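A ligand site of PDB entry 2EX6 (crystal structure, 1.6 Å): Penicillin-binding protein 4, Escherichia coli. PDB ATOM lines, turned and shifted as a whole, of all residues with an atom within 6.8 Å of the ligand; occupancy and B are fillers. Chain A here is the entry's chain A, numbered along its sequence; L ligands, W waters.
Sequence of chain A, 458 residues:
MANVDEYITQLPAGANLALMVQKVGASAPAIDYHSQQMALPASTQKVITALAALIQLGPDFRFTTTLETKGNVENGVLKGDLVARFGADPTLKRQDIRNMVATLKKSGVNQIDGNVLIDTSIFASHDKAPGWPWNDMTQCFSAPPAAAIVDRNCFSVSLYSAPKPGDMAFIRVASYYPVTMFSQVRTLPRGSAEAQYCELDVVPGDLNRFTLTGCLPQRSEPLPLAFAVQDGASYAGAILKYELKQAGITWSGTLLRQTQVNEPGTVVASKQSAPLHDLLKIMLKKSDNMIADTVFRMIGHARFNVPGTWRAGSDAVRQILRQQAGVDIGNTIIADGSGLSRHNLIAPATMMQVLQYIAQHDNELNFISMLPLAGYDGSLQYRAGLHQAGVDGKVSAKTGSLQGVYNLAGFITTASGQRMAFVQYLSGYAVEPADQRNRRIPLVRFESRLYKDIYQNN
O4 of the ligand sits close to N of Ser 43 (2.9 Å). A carbon (C15) of the ligand is covalently linked to the side-chain hydroxyl of Ser 43. The backbone NH (N) of Ser 401 lies within hydrogen-bond range of an oxygen (O4) of the ligand. N1 of the ligand sits at hydrogen-bond distance from O of Ser 401, at 3.0 Å. The side-chain amide nitrogen (ND2) of Asn 289 is in hydrogen-bond range of an oxygen (O3) of the ligand, 3.0 Å away. OG of Ser 287 is in hydrogen-bond range of N2 of the ligand.
The side-chain hydroxyl (OG) of Ser 287 sits at hydrogen-bond distance from the side-chain hydroxyl (OG) of Ser 43, 3.1 Å away. The side-chain hydroxyl (OG) of Ser 43 is in hydrogen-bond range of the side-chain amino group (NZ) of Lys 46, at 2.9 Å. ND2 of Asn 289 sits at hydrogen-bond distance from O of Phe 141, 2.9 Å away. OD1 of Asn 289 lies within hydrogen-bond range of NZ of Lys 46, at 2.8 Å. OG of Ser 287 sits at hydrogen-bond distance from NZ of Lys 46 (3.2 Å). The side-chain amino group (NZ) of Lys 398 is in hydrogen-bond range of the side-chain hydroxyl (OG) of Ser 287 (2.7 Å). N of Leu 340 is in hydrogen-bond range of OG of Ser 338.
Merely in contact with the ligand: Ala 42 (3.7 Å), Phe 141 (3.4 Å), Lys 286 (3.7 Å), Leu 340 (3.3 Å) and Gly 400 (3.7 Å). Hydrophobic or aromatic side chains that line the ligand: Ala 42, Phe 141 and Leu 340. Within 4 Å of the ligand: Ala 42, Ser 43, Phe 141, Lys 286, Ser 287, Asn 289, Leu 340, Gly 400 and Ser 401. The nearest printed residue that does not touch the ligand is Leu 402 (4.01 Å).
Water W5 lies within hydrogen-bond range of O1 of the ligand (2.7 Å), OG1 of Thr 399 (2.7 Å) and OG of Ser 401 (3.4 Å). Water W1 bridges OG of Ser 379 and O1 of the ligand. Water W4 lies within hydrogen-bond range of OG1 of Thr 399 (2.9 Å), N2 of the ligand (2.9 Å), N of Ser 401 (3.1 Å) and N of Gly 400 (3.4 Å).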
ATOM      1  N   PRO A  41      -2.216  18.958 -11.574  1.00  0.00           N
ATOM      2  CA  PRO A  41      -2.268  19.319 -12.998  1.00  0.00           C
ATOM      3  C   PRO A  41      -1.105  18.838 -13.859  1.00  0.00           C
ATOM      4  O   PRO A  41      -1.220  18.731 -15.088  1.00  0.00           O
ATOM      5  CB  PRO A  41      -2.306  20.853 -12.956  1.00  0.00           C
ATOM      6  CG  PRO A  41      -1.477  21.284 -11.728  1.00  0.00           C
ATOM      7  CD  PRO A  41      -1.830  20.121 -10.751  1.00  0.00           C
ATOM      8  N   ALA A  42       0.045  18.579 -13.225  1.00  0.00           N
ATOM      9  CA  ALA A  42       1.280  18.203 -13.926  1.00  0.00           C
ATOM     10  C   ALA A  42       1.531  19.286 -14.990  1.00  0.00           C
ATOM     11  O   ALA A  42       1.257  20.424 -14.715  1.00  0.00           O
ATOM     12  CB  ALA A  42       1.238  16.781 -14.487  1.00  0.00           C
ATOM     13  N   SER A  43       2.019  18.900 -16.165  1.00  0.00           N
ATOM     14  CA  SER A  43       2.444  19.915 -17.175  1.00  0.00           C
ATOM     15  C   SER A  43       1.303  20.740 -17.774  1.00  0.00           C
ATOM     16  O   SER A  43       1.573  21.721 -18.466  1.00  0.00           O
ATOM     17  CB  SER A  43       3.251  19.252 -18.295  1.00  0.00           C
ATOM     18  OG  SER A  43       4.577  18.995 -17.866  1.00  0.00           O
ATOM     19  N   THR A  44       0.051  20.403 -17.455  1.00  0.00           N
ATOM     20  CA  THR A  44      -1.026  21.313 -17.912  1.00  0.00           C
ATOM     21  C   THR A  44      -0.925  22.678 -17.217  1.00  0.00           C
ATOM     22  O   THR A  44      -1.508  23.651 -17.649  1.00  0.00           O
ATOM     23  CB  THR A  44      -2.463  20.729 -17.779  1.00  0.00           C
ATOM     24  OG1 THR A  44      -2.784  20.575 -16.386  1.00  0.00           O
ATOM     25  CG2 THR A  44      -2.539  19.340 -18.403  1.00  0.00           C
ATOM     26  N   LYS A  46       1.376  24.583 -17.439  1.00  0.00           N
ATOM     27  CA  LYS A  46       2.057  25.435 -18.426  1.00  0.00           C
ATOM     28  C   LYS A  46       1.058  26.287 -19.190  1.00  0.00           C
ATOM     29  O   LYS A  46       1.425  27.358 -19.674  1.00  0.00           O
ATOM     30  CB  LYS A  46       2.886  24.572 -19.362  1.00  0.00           C
ATOM     31  CG  LYS A  46       4.138  24.006 -18.635  1.00  0.00           C
ATOM     32  CD  LYS A  46       4.890  23.168 -19.630  1.00  0.00           C
ATOM     33  CE  LYS A  46       6.184  22.736 -19.033  1.00  0.00           C
ATOM     34  NZ  LYS A  46       6.003  21.406 -18.510  1.00  0.00           N
ATOM     35  N   ASP A 136      14.456  13.461  -8.161  1.00  0.00           N
ATOM     36  CA  ASP A 136      14.558  13.824  -9.599  1.00  0.00           C
ATOM     37  C   ASP A 136      15.518  14.998  -9.840  1.00  0.00           C
ATOM     38  O   ASP A 136      15.732  15.408 -11.008  1.00  0.00           O
ATOM     39  CB  ASP A 136      13.173  14.162 -10.186  1.00  0.00           C
ATOM     40  CG  ASP A 136      12.254  12.966 -10.295  1.00  0.00           C
ATOM     41  OD1 ASP A 136      12.724  11.827 -10.566  1.00  0.00           O
ATOM     42  OD2 ASP A 136      10.996  13.097 -10.152  1.00  0.00           O
ATOM     43  N   GLN A 139      18.102  14.711 -12.449  1.00  0.00           N
ATOM     44  CA  GLN A 139      17.661  14.455 -13.834  1.00  0.00           C
ATOM     45  C   GLN A 139      17.481  15.753 -14.591  1.00  0.00           C
ATOM     46  O   GLN A 139      16.996  16.760 -14.031  1.00  0.00           O
ATOM     47  CB  GLN A 139      16.326  13.720 -13.842  1.00  0.00           C
ATOM     48  CG  GLN A 139      16.446  12.275 -13.420  1.00  0.00           C
ATOM     49  CD  GLN A 139      16.424  11.413 -14.623  1.00  0.00           C
ATOM     50  OE1 GLN A 139      17.430  11.303 -15.330  1.00  0.00           O
ATOM     51  NE2 GLN A 139      15.269  10.830 -14.934  1.00  0.00           N
ATOM     52  N   PHE A 141      15.319  16.789 -16.659  1.00  0.00           N
ATOM     53  CA  PHE A 141      13.932  17.324 -16.755  1.00  0.00           C
ATOM     54  C   PHE A 141      13.557  18.145 -15.524  1.00  0.00           C
ATOM     55  O   PHE A 141      12.602  18.957 -15.571  1.00  0.00           O
ATOM     56  CB  PHE A 141      12.873  16.230 -17.000  1.00  0.00           C
ATOM     57  CG  PHE A 141      12.629  15.318 -15.820  1.00  0.00           C
ATOM     58  CD1 PHE A 141      11.856  15.762 -14.728  1.00  0.00           C
ATOM     59  CD2 PHE A 141      13.051  14.006 -15.863  1.00  0.00           C
ATOM     60  CE1 PHE A 141      11.588  14.872 -13.670  1.00  0.00           C
ATOM     61  CE2 PHE A 141      12.806  13.149 -14.807  1.00  0.00           C
ATOM     62  CZ  PHE A 141      12.056  13.588 -13.720  1.00  0.00           C
ATOM     63  N   SER A 142      14.346  18.000 -14.459  1.00  0.00           N
ATOM     64  CA  SER A 142      14.114  18.734 -13.238  1.00  0.00           C
ATOM     65  C   SER A 142      15.339  19.589 -12.839  1.00  0.00           C
ATOM     66  O   SER A 142      15.505  19.998 -11.685  1.00  0.00           O
ATOM     67  CB  SER A 142      13.773  17.754 -12.095  1.00  0.00           C
ATOM     68  OG  SER A 142      13.404  18.519 -10.925  1.00  0.00           O
ATOM     69  N   LYS A 286       6.482  21.191 -26.667  1.00  0.00           N
ATOM     70  CA  LYS A 286       7.436  20.167 -26.263  1.00  0.00           C
ATOM     71  C   LYS A 286       7.331  19.894 -24.780  1.00  0.00           C
ATOM     72  O   LYS A 286       7.922  18.920 -24.254  1.00  0.00           O
ATOM     73  CB  LYS A 286       8.853  20.645 -26.609  1.00  0.00           C
ATOM     74  CG  LYS A 286       9.117  20.833 -28.110  1.00  0.00           C
ATOM     75  CD  LYS A 286       9.367  19.473 -28.764  1.00  0.00           C
ATOM     76  CE  LYS A 286      10.010  19.613 -30.147  1.00  0.00           C
ATOM     77  NZ  LYS A 286      11.266  20.429 -30.107  1.00  0.00           N
ATOM     78  N   SER A 287       6.570  20.733 -24.085  1.00  0.00           N
ATOM     79  CA  SER A 287       6.377  20.640 -22.608  1.00  0.00           C
ATOM     80  C   SER A 287       7.723  20.870 -21.901  1.00  0.00           C
ATOM     81  O   SER A 287       8.201  20.010 -21.158  1.00  0.00           O
ATOM     82  CB  SER A 287       5.769  19.295 -22.181  1.00  0.00           C
ATOM     83  OG  SER A 287       5.141  19.466 -20.901  1.00  0.00           O
ATOM     84  N   ASP A 288       8.306  22.049 -22.118  1.00  0.00           N
ATOM     85  CA  ASP A 288       9.656  22.349 -21.640  1.00  0.00           C
ATOM     86  C   ASP A 288       9.592  22.916 -20.235  1.00  0.00           C
ATOM     87  O   ASP A 288       9.250  24.074 -20.017  1.00  0.00           O
ATOM     88  CB  ASP A 288      10.305  23.356 -22.629  1.00  0.00           C
ATOM     89  CG  ASP A 288      11.776  23.548 -22.388  1.00  0.00           C
ATOM     90  OD1 ASP A 288      12.182  23.732 -21.213  1.00  0.00           O
ATOM     91  OD2 ASP A 288      12.613  23.531 -23.317  1.00  0.00           O
ATOM     92  N   ASN A 289       9.943  22.083 -19.252  1.00  0.00           N
ATOM     93  CA  ASN A 289       9.908  22.499 -17.826  1.00  0.00           C
ATOM     94  C   ASN A 289      10.748  23.736 -17.522  1.00  0.00           C
ATOM     95  O   ASN A 289      10.369  24.586 -16.709  1.00  0.00           O
ATOM     96  CB  ASN A 289      10.364  21.322 -16.927  1.00  0.00           C
ATOM     97  CG  ASN A 289       9.383  20.127 -16.913  1.00  0.00           C
ATOM     98  OD1 ASN A 289       8.153  20.269 -17.129  1.00  0.00           O
ATOM     99  ND2 ASN A 289       9.920  18.936 -16.606  1.00  0.00           N
ATOM    100  N   SER A 338       5.986  24.980 -14.318  1.00  0.00           N
ATOM    101  CA  SER A 338       6.059  23.770 -15.123  1.00  0.00           C
ATOM    102  C   SER A 338       5.015  22.709 -14.762  1.00  0.00           C
ATOM    103  O   SER A 338       4.728  21.806 -15.582  1.00  0.00           O
ATOM    104  CB  SER A 338       7.445  23.140 -14.989  1.00  0.00           C
ATOM    105  OG  SER A 338       7.704  22.866 -13.605  1.00  0.00           O
ATOM    106  N   GLY A 339       4.519  22.763 -13.520  1.00  0.00           N
ATOM    107  CA  GLY A 339       3.708  21.672 -13.009  1.00  0.00           C
ATOM    108  C   GLY A 339       4.497  20.519 -12.385  1.00  0.00           C
ATOM    109  O   GLY A 339       3.908  19.497 -12.042  1.00  0.00           O
ATOM    110  N   LEU A 340       5.833  20.654 -12.231  1.00  0.00           N
ATOM    111  CA  LEU A 340       6.619  19.616 -11.545  1.00  0.00           C
ATOM    112  C   LEU A 340       6.150  19.395 -10.095  1.00  0.00           C
ATOM    113  O   LEU A 340       6.191  18.265  -9.578  1.00  0.00           O
ATOM    114  CB  LEU A 340       8.113  19.975 -11.504  1.00  0.00           C
ATOM    115  CG  LEU A 340       8.845  19.707 -12.811  1.00  0.00           C
ATOM    116  CD1 LEU A 340      10.261  20.328 -12.748  1.00  0.00           C
ATOM    117  CD2 LEU A 340       8.930  18.187 -13.104  1.00  0.00           C
ATOM    118  N   SER A 379       3.585  17.201 -28.350  1.00  0.00           N
ATOM    119  CA  SER A 379       3.291  16.025 -27.556  1.00  0.00           C
ATOM    120  C   SER A 379       2.172  15.161 -28.120  1.00  0.00           C
ATOM    121  O   SER A 379       2.062  13.994 -27.717  1.00  0.00           O
ATOM    122  CB  SER A 379       3.008  16.466 -26.117  1.00  0.00           C
ATOM    123  OG  SER A 379       3.999  17.397 -25.722  1.00  0.00           O
ATOM    124  N   LYS A 398      -2.825  20.648 -24.234  1.00  0.00           N
ATOM    125  CA  LYS A 398      -1.586  20.469 -23.464  1.00  0.00           C
ATOM    126  C   LYS A 398      -1.657  19.190 -22.611  1.00  0.00           C
ATOM    127  O   LYS A 398      -2.646  18.947 -21.921  1.00  0.00           O
ATOM    128  CB  LYS A 398      -1.402  21.666 -22.549  1.00  0.00           C
ATOM    129  CG  LYS A 398      -0.096  21.625 -21.739  1.00  0.00           C
ATOM    130  CD  LYS A 398       1.131  21.679 -22.694  1.00  0.00           C
ATOM    131  CE  LYS A 398       2.447  21.373 -21.929  1.00  0.00           C
ATOM    132  NZ  LYS A 398       2.622  19.927 -21.734  1.00  0.00           N
ATOM    133  N   THR A 399      -0.621  18.377 -22.673  1.00  0.00           N
ATOM    134  CA  THR A 399      -0.568  17.145 -21.879  1.00  0.00           C
ATOM    135  C   THR A 399      -0.013  17.469 -20.475  1.00  0.00           C
ATOM    136  O   THR A 399       0.677  18.464 -20.258  1.00  0.00           O
ATOM    137  CB  THR A 399       0.331  16.092 -22.521  1.00  0.00           C
ATOM    138  OG1 THR A 399       1.632  16.680 -22.731  1.00  0.00           O
ATOM    139  CG2 THR A 399      -0.168  15.679 -23.940  1.00  0.00           C
ATOM    140  N   GLY A 400      -0.325  16.580 -19.518  1.00  0.00           N
ATOM    141  CA  GLY A 400       0.331  16.613 -18.189  1.00  0.00           C
ATOM    142  C   GLY A 400       0.651  15.159 -17.874  1.00  0.00           C
ATOM    143  O   GLY A 400      -0.247  14.362 -17.740  1.00  0.00           O
ATOM    144  N   SER A 401       1.933  14.815 -17.830  1.00  0.00           N
ATOM    145  CA  SER A 401       2.337  13.387 -17.990  1.00  0.00           C
ATOM    146  C   SER A 401       3.397  12.990 -16.987  1.00  0.00           C
ATOM    147  O   SER A 401       4.450  13.645 -16.882  1.00  0.00           O
ATOM    148  CB  SER A 401       2.861  13.109 -19.414  1.00  0.00           C
ATOM    149  OG  SER A 401       1.822  13.139 -20.400  1.00  0.00           O
ATOM    150  N   LEU A 402       3.104  11.933 -16.223  1.00  0.00           N
ATOM    151  CA  LEU A 402       4.085  11.268 -15.352  1.00  0.00           C
ATOM    152  C   LEU A 402       3.459   9.923 -14.949  1.00  0.00           C
ATOM    153  O   LEU A 402       2.334   9.642 -15.349  1.00  0.00           O
ATOM    154  CB  LEU A 402       4.440  12.110 -14.107  1.00  0.00           C
ATOM    155  CG  LEU A 402       3.361  12.373 -13.058  1.00  0.00           C
ATOM    156  CD1 LEU A 402       3.926  12.472 -11.654  1.00  0.00           C
ATOM    157  CD2 LEU A 402       2.634  13.668 -13.407  1.00  0.00           C
ATOM    158  N   GLN A 403       4.182   9.115 -14.160  1.00  0.00           N
ATOM    159  CA  GLN A 403       3.699   7.764 -13.833  1.00  0.00           C
ATOM    160  C   GLN A 403       2.248   7.779 -13.344  1.00  0.00           C
ATOM    161  O   GLN A 403       1.912   8.439 -12.356  1.00  0.00           O
ATOM    162  CB  GLN A 403       4.604   7.074 -12.806  1.00  0.00           C
ATOM    163  CG  GLN A 403       4.316   5.554 -12.682  1.00  0.00           C
ATOM    164  CD  GLN A 403       4.020   5.106 -11.243  1.00  0.00           C
ATOM    165  OE1 GLN A 403       4.669   4.177 -10.725  1.00  0.00           O
ATOM    166  NE2 GLN A 403       3.049   5.759 -10.595  1.00  0.00           N
HETATM  167  C1  LIG L   1       8.219  11.454 -18.055  1.00  0.00           C
HETATM  168  C2  LIG L   1       8.224  13.293 -16.512  1.00  0.00           C
HETATM  169  C3  LIG L   1       8.176  15.433 -20.519  1.00  0.00           C
HETATM  170  N1  LIG L   1       6.437  15.932 -16.939  1.00  0.00           N
HETATM  171  C4  LIG L   1       6.053  14.625 -21.583  1.00  0.00           C
HETATM  172  N2  LIG L   1       5.959  16.428 -19.959  1.00  0.00           N
HETATM  173  C5  LIG L   1       7.502  14.239 -15.582  1.00  0.00           C
HETATM  174  C6  LIG L   1       8.540  16.120 -21.854  1.00  0.00           C
HETATM  175  C7  LIG L   1       7.473  15.663 -16.148  1.00  0.00           C
HETATM  176  C8  LIG L   1       7.528  12.313 -17.217  1.00  0.00           C
HETATM  177  C9  LIG L   1       9.592  11.546 -18.206  1.00  0.00           C
HETATM  178  C10 LIG L   1      10.298  12.507 -17.496  1.00  0.00           C
HETATM  179  C11 LIG L   1       9.624  13.391 -16.659  1.00  0.00           C
HETATM  180  C12 LIG L   1       6.655  15.167 -20.302  1.00  0.00           C
HETATM  181  C13 LIG L   1       6.769  17.221 -19.015  1.00  0.00           C
HETATM  182  C14 LIG L   1       6.260  17.260 -17.556  1.00  0.00           C
HETATM  183  C15 LIG L   1       4.778  17.673 -17.524  1.00  0.00           C
HETATM  184  C16 LIG L   1       9.068  14.199 -20.336  1.00  0.00           C
HETATM  185  N3  LIG L   1       8.250  14.338 -14.331  1.00  0.00           N
HETATM  186  O1  LIG L   1       5.486  15.461 -22.338  1.00  0.00           O
HETATM  187  O2  LIG L   1       6.210  13.412 -21.805  1.00  0.00           O
HETATM  188  O3  LIG L   1       8.362  16.463 -15.872  1.00  0.00           O
HETATM  189  O4  LIG L   1       3.894  16.930 -17.109  1.00  0.00           O
HETATM  190  S1  LIG L   1       8.459  16.597 -19.178  1.00  0.00           S
HETATM  191  O   HOH W   1       5.971  15.960 -24.958  1.00  0.00           O
HETATM  192  O   HOH W   2       5.729  11.009 -20.693  1.00  0.00           O
HETATM  193  O   HOH W   3       6.113  15.189 -12.700  1.00  0.00           O
HETATM  194  O   HOH W   4       3.026  16.327 -20.252  1.00  0.00           O
HETATM  195  O   HOH W   5       3.156  14.513 -23.229  1.00  0.00           O
